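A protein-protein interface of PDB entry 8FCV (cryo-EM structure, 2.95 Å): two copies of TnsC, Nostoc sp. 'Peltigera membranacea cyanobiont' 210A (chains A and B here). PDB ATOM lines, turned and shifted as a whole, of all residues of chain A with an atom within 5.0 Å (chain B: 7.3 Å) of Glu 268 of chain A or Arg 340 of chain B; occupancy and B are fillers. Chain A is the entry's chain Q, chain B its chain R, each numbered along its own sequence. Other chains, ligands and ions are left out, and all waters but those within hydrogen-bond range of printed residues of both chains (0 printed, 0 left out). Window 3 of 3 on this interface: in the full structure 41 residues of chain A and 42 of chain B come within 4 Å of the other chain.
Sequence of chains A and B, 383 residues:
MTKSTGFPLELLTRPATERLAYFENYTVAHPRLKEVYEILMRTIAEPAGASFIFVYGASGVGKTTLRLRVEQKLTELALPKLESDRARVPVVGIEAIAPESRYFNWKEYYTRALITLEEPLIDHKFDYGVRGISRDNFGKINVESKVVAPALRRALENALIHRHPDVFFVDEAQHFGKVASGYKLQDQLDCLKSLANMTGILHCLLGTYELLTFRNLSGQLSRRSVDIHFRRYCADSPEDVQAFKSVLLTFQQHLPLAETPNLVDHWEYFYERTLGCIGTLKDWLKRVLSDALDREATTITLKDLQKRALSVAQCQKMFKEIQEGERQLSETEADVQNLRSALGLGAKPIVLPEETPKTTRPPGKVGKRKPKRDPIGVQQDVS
Of the 8 printed residues of chain A, 4 touch a printed residue of chain B.
Hydrophobic or aromatic side chains of chain A that line the printed part of chain B: Trp 267 and Tyr 271.
Among the printed residues, 7 pairs touch across the chains.
Arg 340 of chain B touches just these residues of chain A: Glu 268 (3.0 Å) and Glu 272 (3.4 Å).
Of the printed residues of chain A, Leu 345 of chain B touches Trp 267, Glu 268 and Glu 272.
Printed residues of chain B within 4 Å of Trp 267 of chain A: Leu 345 (3.996 Å).
Printed residues of chain A within 4 Å of Leu 343 of chain B: Tyr 271 (3.7 Å).
Of the printed residues of chain A, Val 336 of chain B touches Glu 272.
Of the printed residues of chain B, Glu 272 of chain A touches Val 336, Arg 340 and Leu 345.
Phe 270 of chain A touches none of the printed residues of chain B.
The nearest residue of chain B that does not touch Glu 268 of chain A is Gly 346 of chain B (5.6 Å).
The nearest printed residue of chain A that does not touch Leu 345 of chain B is Tyr 271 of chain A (4.5 Å).
The backbone carbonyl oxygen (O) of Arg 340 of chain B lies within hydrogen-bond range of the backbone NH (N) of Leu 345 of chain B.
The backbone carbonyl oxygen of Arg 340 of chain B is in hydrogen-bond range of the backbone NH of Gly 346 of chain B (3.0 Å).
OE1 of Glu 268 of chain A is in salt-bridge range of NH1 of Arg 340 of chain B (3.0 Å).
No position is printed for both chains.
Of the 7 pairs that touch across the chains among the printed residues, none has its exchanged pair printed and touching as well.
Among the printed residues, pairs that only touch across the chains: Glu 268 of chain A with Leu 345 of chain B (3.2 Å), Glu 272 of chain A with Arg 340 of chain B (3.4 Å), Glu 272 of chain A with Leu 345 of chain B (3.6 Å), Tyr 271 of chain A with Leu 343 of chain B (3.7 Å), Glu 272 of chain A with Val 336 of chain B (3.96 Å) and Trp 267 of chain A with Leu 345 of chain B (3.996 Å).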
ATOM      1  N   ASP A 265     -20.610  10.408  40.095  1.00  0.00           N
ATOM      2  CA  ASP A 265     -19.750   9.745  39.118  1.00  0.00           C
ATOM      3  C   ASP A 265     -20.177  10.072  37.692  1.00  0.00           C
ATOM      4  O   ASP A 265     -19.343  10.420  36.847  1.00  0.00           O
ATOM      5  CB  ASP A 265     -19.758   8.234  39.347  1.00  0.00           C
ATOM      6  CG  ASP A 265     -18.645   7.525  38.601  1.00  0.00           C
ATOM      7  OD1 ASP A 265     -17.750   8.215  38.068  1.00  0.00           O
ATOM      8  OD2 ASP A 265     -18.664   6.277  38.549  1.00  0.00           O
ATOM      9  N   HIS A 266     -21.473   9.970  37.402  1.00  0.00           N
ATOM     10  CA  HIS A 266     -21.959  10.298  36.067  1.00  0.00           C
ATOM     11  C   HIS A 266     -22.207  11.794  35.935  1.00  0.00           C
ATOM     12  O   HIS A 266     -23.263  12.216  35.448  1.00  0.00           O
ATOM     13  CB  HIS A 266     -23.241   9.520  35.755  1.00  0.00           C
ATOM     14  CG  HIS A 266     -23.286   8.156  36.367  1.00  0.00           C
ATOM     15  ND1 HIS A 266     -22.606   7.081  35.837  1.00  0.00           N
ATOM     16  CD2 HIS A 266     -23.929   7.690  37.463  1.00  0.00           C
ATOM     17  CE1 HIS A 266     -22.829   6.011  36.580  1.00  0.00           C
ATOM     18  NE2 HIS A 266     -23.629   6.354  37.573  1.00  0.00           N
ATOM     19  N   TRP A 267     -21.226  12.605  36.337  1.00  0.00           N
ATOM     20  CA  TRP A 267     -21.383  14.051  36.230  1.00  0.00           C
ATOM     21  C   TRP A 267     -21.389  14.492  34.773  1.00  0.00           C
ATOM     22  O   TRP A 267     -22.133  15.406  34.399  1.00  0.00           O
ATOM     23  CB  TRP A 267     -20.285  14.758  37.030  1.00  0.00           C
ATOM     24  CG  TRP A 267     -18.949  14.855  36.354  1.00  0.00           C
ATOM     25  CD1 TRP A 267     -17.863  14.058  36.574  1.00  0.00           C
ATOM     26  CD2 TRP A 267     -18.537  15.836  35.393  1.00  0.00           C
ATOM     27  NE1 TRP A 267     -16.812  14.461  35.787  1.00  0.00           N
ATOM     28  CE2 TRP A 267     -17.198  15.551  35.055  1.00  0.00           C
ATOM     29  CE3 TRP A 267     -19.173  16.916  34.774  1.00  0.00           C
ATOM     30  CZ2 TRP A 267     -16.485  16.307  34.128  1.00  0.00           C
ATOM     31  CZ3 TRP A 267     -18.464  17.665  33.853  1.00  0.00           C
ATOM     32  CH2 TRP A 267     -17.135  17.358  33.539  1.00  0.00           C
ATOM     33  N   GLU A 268     -20.581  13.842  33.933  1.00  0.00           N
ATOM     34  CA  GLU A 268     -20.595  14.151  32.507  1.00  0.00           C
ATOM     35  C   GLU A 268     -21.955  13.844  31.893  1.00  0.00           C
ATOM     36  O   GLU A 268     -22.496  14.651  31.128  1.00  0.00           O
ATOM     37  CB  GLU A 268     -19.493  13.370  31.794  1.00  0.00           C
ATOM     38  CG  GLU A 268     -18.100  13.626  32.344  1.00  0.00           C
ATOM     39  CD  GLU A 268     -17.005  13.259  31.363  1.00  0.00           C
ATOM     40  OE1 GLU A 268     -17.305  13.125  30.158  1.00  0.00           O
ATOM     41  OE2 GLU A 268     -15.844  13.103  31.796  1.00  0.00           O
ATOM     42  N   TYR A 269     -22.527  12.683  32.220  1.00  0.00           N
ATOM     43  CA  TYR A 269     -23.839  12.336  31.689  1.00  0.00           C
ATOM     44  C   TYR A 269     -24.910  13.296  32.189  1.00  0.00           C
ATOM     45  O   TYR A 269     -25.791  13.708  31.425  1.00  0.00           O
ATOM     46  CB  TYR A 269     -24.200  10.897  32.057  1.00  0.00           C
ATOM     47  CG  TYR A 269     -25.567  10.480  31.564  1.00  0.00           C
ATOM     48  CD1 TYR A 269     -25.942  10.690  30.244  1.00  0.00           C
ATOM     49  CD2 TYR A 269     -26.484   9.886  32.419  1.00  0.00           C
ATOM     50  CE1 TYR A 269     -27.189  10.318  29.787  1.00  0.00           C
ATOM     51  CE2 TYR A 269     -27.736   9.508  31.971  1.00  0.00           C
ATOM     52  CZ  TYR A 269     -28.083   9.726  30.655  1.00  0.00           C
ATOM     53  OH  TYR A 269     -29.327   9.352  30.205  1.00  0.00           O
ATOM     54  N   PHE A 270     -24.858  13.661  33.473  1.00  0.00           N
ATOM     55  CA  PHE A 270     -25.843  14.596  34.008  1.00  0.00           C
ATOM     56  C   PHE A 270     -25.720  15.971  33.363  1.00  0.00           C
ATOM     57  O   PHE A 270     -26.733  16.639  33.133  1.00  0.00           O
ATOM     58  CB  PHE A 270     -25.701  14.704  35.525  1.00  0.00           C
ATOM     59  CG  PHE A 270     -26.498  13.678  36.280  1.00  0.00           C
ATOM     60  CD1 PHE A 270     -27.880  13.716  36.274  1.00  0.00           C
ATOM     61  CD2 PHE A 270     -25.864  12.682  37.003  1.00  0.00           C
ATOM     62  CE1 PHE A 270     -28.617  12.775  36.966  1.00  0.00           C
ATOM     63  CE2 PHE A 270     -26.594  11.739  37.698  1.00  0.00           C
ATOM     64  CZ  PHE A 270     -27.973  11.786  37.680  1.00  0.00           C
ATOM     65  N   TYR A 271     -24.496  16.407  33.064  1.00  0.00           N
ATOM     66  CA  TYR A 271     -24.303  17.697  32.413  1.00  0.00           C
ATOM     67  C   TYR A 271     -24.697  17.666  30.942  1.00  0.00           C
ATOM     68  O   TYR A 271     -25.112  18.695  30.397  1.00  0.00           O
ATOM     69  CB  TYR A 271     -22.845  18.140  32.555  1.00  0.00           C
ATOM     70  CG  TYR A 271     -22.601  19.576  32.157  1.00  0.00           C
ATOM     71  CD1 TYR A 271     -22.303  19.913  30.844  1.00  0.00           C
ATOM     72  CD2 TYR A 271     -22.675  20.598  33.095  1.00  0.00           C
ATOM     73  CE1 TYR A 271     -22.082  21.221  30.476  1.00  0.00           C
ATOM     74  CE2 TYR A 271     -22.454  21.910  32.734  1.00  0.00           C
ATOM     75  CZ  TYR A 271     -22.159  22.217  31.423  1.00  0.00           C
ATOM     76  OH  TYR A 271     -21.938  23.523  31.055  1.00  0.00           O
ATOM     77  N   GLU A 272     -24.572  16.509  30.288  1.00  0.00           N
ATOM     78  CA  GLU A 272     -24.853  16.433  28.857  1.00  0.00           C
ATOM     79  C   GLU A 272     -26.311  16.760  28.553  1.00  0.00           C
ATOM     80  O   GLU A 272     -26.605  17.486  27.596  1.00  0.00           O
ATOM     81  CB  GLU A 272     -24.491  15.044  28.328  1.00  0.00           C
ATOM     82  CG  GLU A 272     -25.321  14.584  27.141  1.00  0.00           C
ATOM     83  CD  GLU A 272     -25.137  13.109  26.841  1.00  0.00           C
ATOM     84  OE1 GLU A 272     -23.979  12.641  26.841  1.00  0.00           O
ATOM     85  OE2 GLU A 272     -26.149  12.418  26.600  1.00  0.00           O
ATOM     86  N   ALA B 334     -23.833   9.446  16.831  1.00  0.00           N
ATOM     87  CA  ALA B 334     -23.127  10.537  16.169  1.00  0.00           C
ATOM     88  C   ALA B 334     -23.663  11.888  16.621  1.00  0.00           C
ATOM     89  O   ALA B 334     -22.895  12.839  16.809  1.00  0.00           O
ATOM     90  CB  ALA B 334     -23.239  10.393  14.652  1.00  0.00           C
ATOM     91  N   ASP B 335     -24.983  11.994  16.796  1.00  0.00           N
ATOM     92  CA  ASP B 335     -25.577  13.227  17.300  1.00  0.00           C
ATOM     93  C   ASP B 335     -25.219  13.487  18.756  1.00  0.00           C
ATOM     94  O   ASP B 335     -25.427  14.602  19.246  1.00  0.00           O
ATOM     95  CB  ASP B 335     -27.098  13.183  17.138  1.00  0.00           C
ATOM     96  CG  ASP B 335     -27.524  12.886  15.715  1.00  0.00           C
ATOM     97  OD1 ASP B 335     -26.790  13.268  14.781  1.00  0.00           O
ATOM     98  OD2 ASP B 335     -28.595  12.270  15.530  1.00  0.00           O
ATOM     99  N   VAL B 336     -24.694  12.484  19.463  1.00  0.00           N
ATOM    100  CA  VAL B 336     -24.300  12.680  20.853  1.00  0.00           C
ATOM    101  C   VAL B 336     -22.919  13.322  20.932  1.00  0.00           C
ATOM    102  O   VAL B 336     -22.681  14.223  21.744  1.00  0.00           O
ATOM    103  CB  VAL B 336     -24.346  11.343  21.616  1.00  0.00           C
ATOM    104  CG1 VAL B 336     -23.856  11.525  23.044  1.00  0.00           C
ATOM    105  CG2 VAL B 336     -25.753  10.772  21.599  1.00  0.00           C
ATOM    106  N   GLN B 337     -21.991  12.868  20.086  1.00  0.00           N
ATOM    107  CA  GLN B 337     -20.600  13.300  20.198  1.00  0.00           C
ATOM    108  C   GLN B 337     -20.455  14.800  19.968  1.00  0.00           C
ATOM    109  O   GLN B 337     -19.783  15.493  20.741  1.00  0.00           O
ATOM    110  CB  GLN B 337     -19.730  12.517  19.215  1.00  0.00           C
ATOM    111  CG  GLN B 337     -19.912  11.006  19.279  1.00  0.00           C
ATOM    112  CD  GLN B 337     -20.014  10.486  20.702  1.00  0.00           C
ATOM    113  OE1 GLN B 337     -21.108  10.348  21.251  1.00  0.00           O
ATOM    114  NE2 GLN B 337     -18.868  10.195  21.308  1.00  0.00           N
ATOM    115  N   ASN B 338     -21.075  15.324  18.907  1.00  0.00           N
ATOM    116  CA  ASN B 338     -20.975  16.757  18.642  1.00  0.00           C
ATOM    117  C   ASN B 338     -21.631  17.564  19.753  1.00  0.00           C
ATOM    118  O   ASN B 338     -21.132  18.630  20.132  1.00  0.00           O
ATOM    119  CB  ASN B 338     -21.598  17.099  17.289  1.00  0.00           C
ATOM    120  CG  ASN B 338     -22.840  16.291  17.004  1.00  0.00           C
ATOM    121  OD1 ASN B 338     -23.176  15.376  17.750  1.00  0.00           O
ATOM    122  ND2 ASN B 338     -23.530  16.625  15.920  1.00  0.00           N
ATOM    123  N   LEU B 339     -22.749  17.072  20.289  1.00  0.00           N
ATOM    124  CA  LEU B 339     -23.372  17.725  21.436  1.00  0.00           C
ATOM    125  C   LEU B 339     -22.421  17.748  22.625  1.00  0.00           C
ATOM    126  O   LEU B 339     -22.300  18.761  23.322  1.00  0.00           O
ATOM    127  CB  LEU B 339     -24.677  17.012  21.798  1.00  0.00           C
ATOM    128  CG  LEU B 339     -25.489  17.595  22.956  1.00  0.00           C
ATOM    129  CD1 LEU B 339     -25.937  19.014  22.643  1.00  0.00           C
ATOM    130  CD2 LEU B 339     -26.685  16.708  23.266  1.00  0.00           C
ATOM    131  N   ARG B 340     -21.732  16.631  22.870  1.00  0.00           N
ATOM    132  CA  ARG B 340     -20.670  16.623  23.871  1.00  0.00           C
ATOM    133  C   ARG B 340     -19.519  17.526  23.452  1.00  0.00           C
ATOM    134  O   ARG B 340     -18.932  18.228  24.286  1.00  0.00           O
ATOM    135  CB  ARG B 340     -20.178  15.193  24.100  1.00  0.00           C
ATOM    136  CG  ARG B 340     -21.253  14.239  24.594  1.00  0.00           C
ATOM    137  CD  ARG B 340     -20.864  13.594  25.913  1.00  0.00           C
ATOM    138  NE  ARG B 340     -19.456  13.216  25.942  1.00  0.00           N
ATOM    139  CZ  ARG B 340     -18.820  12.770  27.016  1.00  0.00           C
ATOM    140  NH1 ARG B 340     -19.439  12.632  28.177  1.00  0.00           N
ATOM    141  NH2 ARG B 340     -17.532  12.454  26.923  1.00  0.00           N
ATOM    142  N   SER B 341     -19.178  17.520  22.162  1.00  0.00           N
ATOM    143  CA  SER B 341     -18.080  18.350  21.675  1.00  0.00           C
ATOM    144  C   SER B 341     -18.438  19.830  21.731  1.00  0.00           C
ATOM    145  O   SER B 341     -17.618  20.660  22.140  1.00  0.00           O
ATOM    146  CB  SER B 341     -17.710  17.940  20.249  1.00  0.00           C
ATOM    147  OG  SER B 341     -17.405  16.557  20.180  1.00  0.00           O
ATOM    148  N   ALA B 342     -19.657  20.180  21.311  1.00  0.00           N
ATOM    149  CA  ALA B 342     -20.060  21.583  21.300  1.00  0.00           C
ATOM    150  C   ALA B 342     -20.088  22.162  22.710  1.00  0.00           C
ATOM    151  O   ALA B 342     -19.661  23.303  22.928  1.00  0.00           O
ATOM    152  CB  ALA B 342     -21.422  21.733  20.627  1.00  0.00           C
ATOM    153  N   LEU B 343     -20.584  21.392  23.678  1.00  0.00           N
ATOM    154  CA  LEU B 343     -20.580  21.828  25.068  1.00  0.00           C
ATOM    155  C   LEU B 343     -19.180  21.886  25.663  1.00  0.00           C
ATOM    156  O   LEU B 343     -19.008  22.462  26.742  1.00  0.00           O
ATOM    157  CB  LEU B 343     -21.445  20.895  25.919  1.00  0.00           C
ATOM    158  CG  LEU B 343     -22.955  21.122  25.934  1.00  0.00           C
ATOM    159  CD1 LEU B 343     -23.680  19.794  26.079  1.00  0.00           C
ATOM    160  CD2 LEU B 343     -23.339  22.069  27.059  1.00  0.00           C
ATOM    161  N   GLY B 344     -18.183  21.312  24.994  1.00  0.00           N
ATOM    162  CA  GLY B 344     -16.873  21.146  25.579  1.00  0.00           C
ATOM    163  C   GLY B 344     -16.757  19.970  26.519  1.00  0.00           C
ATOM    164  O   GLY B 344     -15.685  19.763  27.101  1.00  0.00           O
ATOM    165  N   LEU B 345     -17.828  19.194  26.688  1.00  0.00           N
ATOM    166  CA  LEU B 345     -17.836  18.050  27.588  1.00  0.00           C
ATOM    167  C   LEU B 345     -17.015  16.881  27.058  1.00  0.00           C
ATOM    168  O   LEU B 345     -16.678  15.981  27.834  1.00  0.00           O
ATOM    169  CB  LEU B 345     -19.284  17.621  27.838  1.00  0.00           C
ATOM    170  CG  LEU B 345     -19.588  16.371  28.661  1.00  0.00           C
ATOM    171  CD1 LEU B 345     -19.036  16.519  30.068  1.00  0.00           C
ATOM    172  CD2 LEU B 345     -21.080  16.117  28.688  1.00  0.00           C
ATOM    173  N   GLY B 346     -16.671  16.885  25.772  1.00  0.00           N
ATOM    174  CA  GLY B 346     -15.893  15.794  25.218  1.00  0.00           C
ATOM    175  C   GLY B 346     -14.564  15.628  25.929  1.00  0.00           C
ATOM    176  O   GLY B 346     -14.008  16.574  26.490  1.00  0.00           O
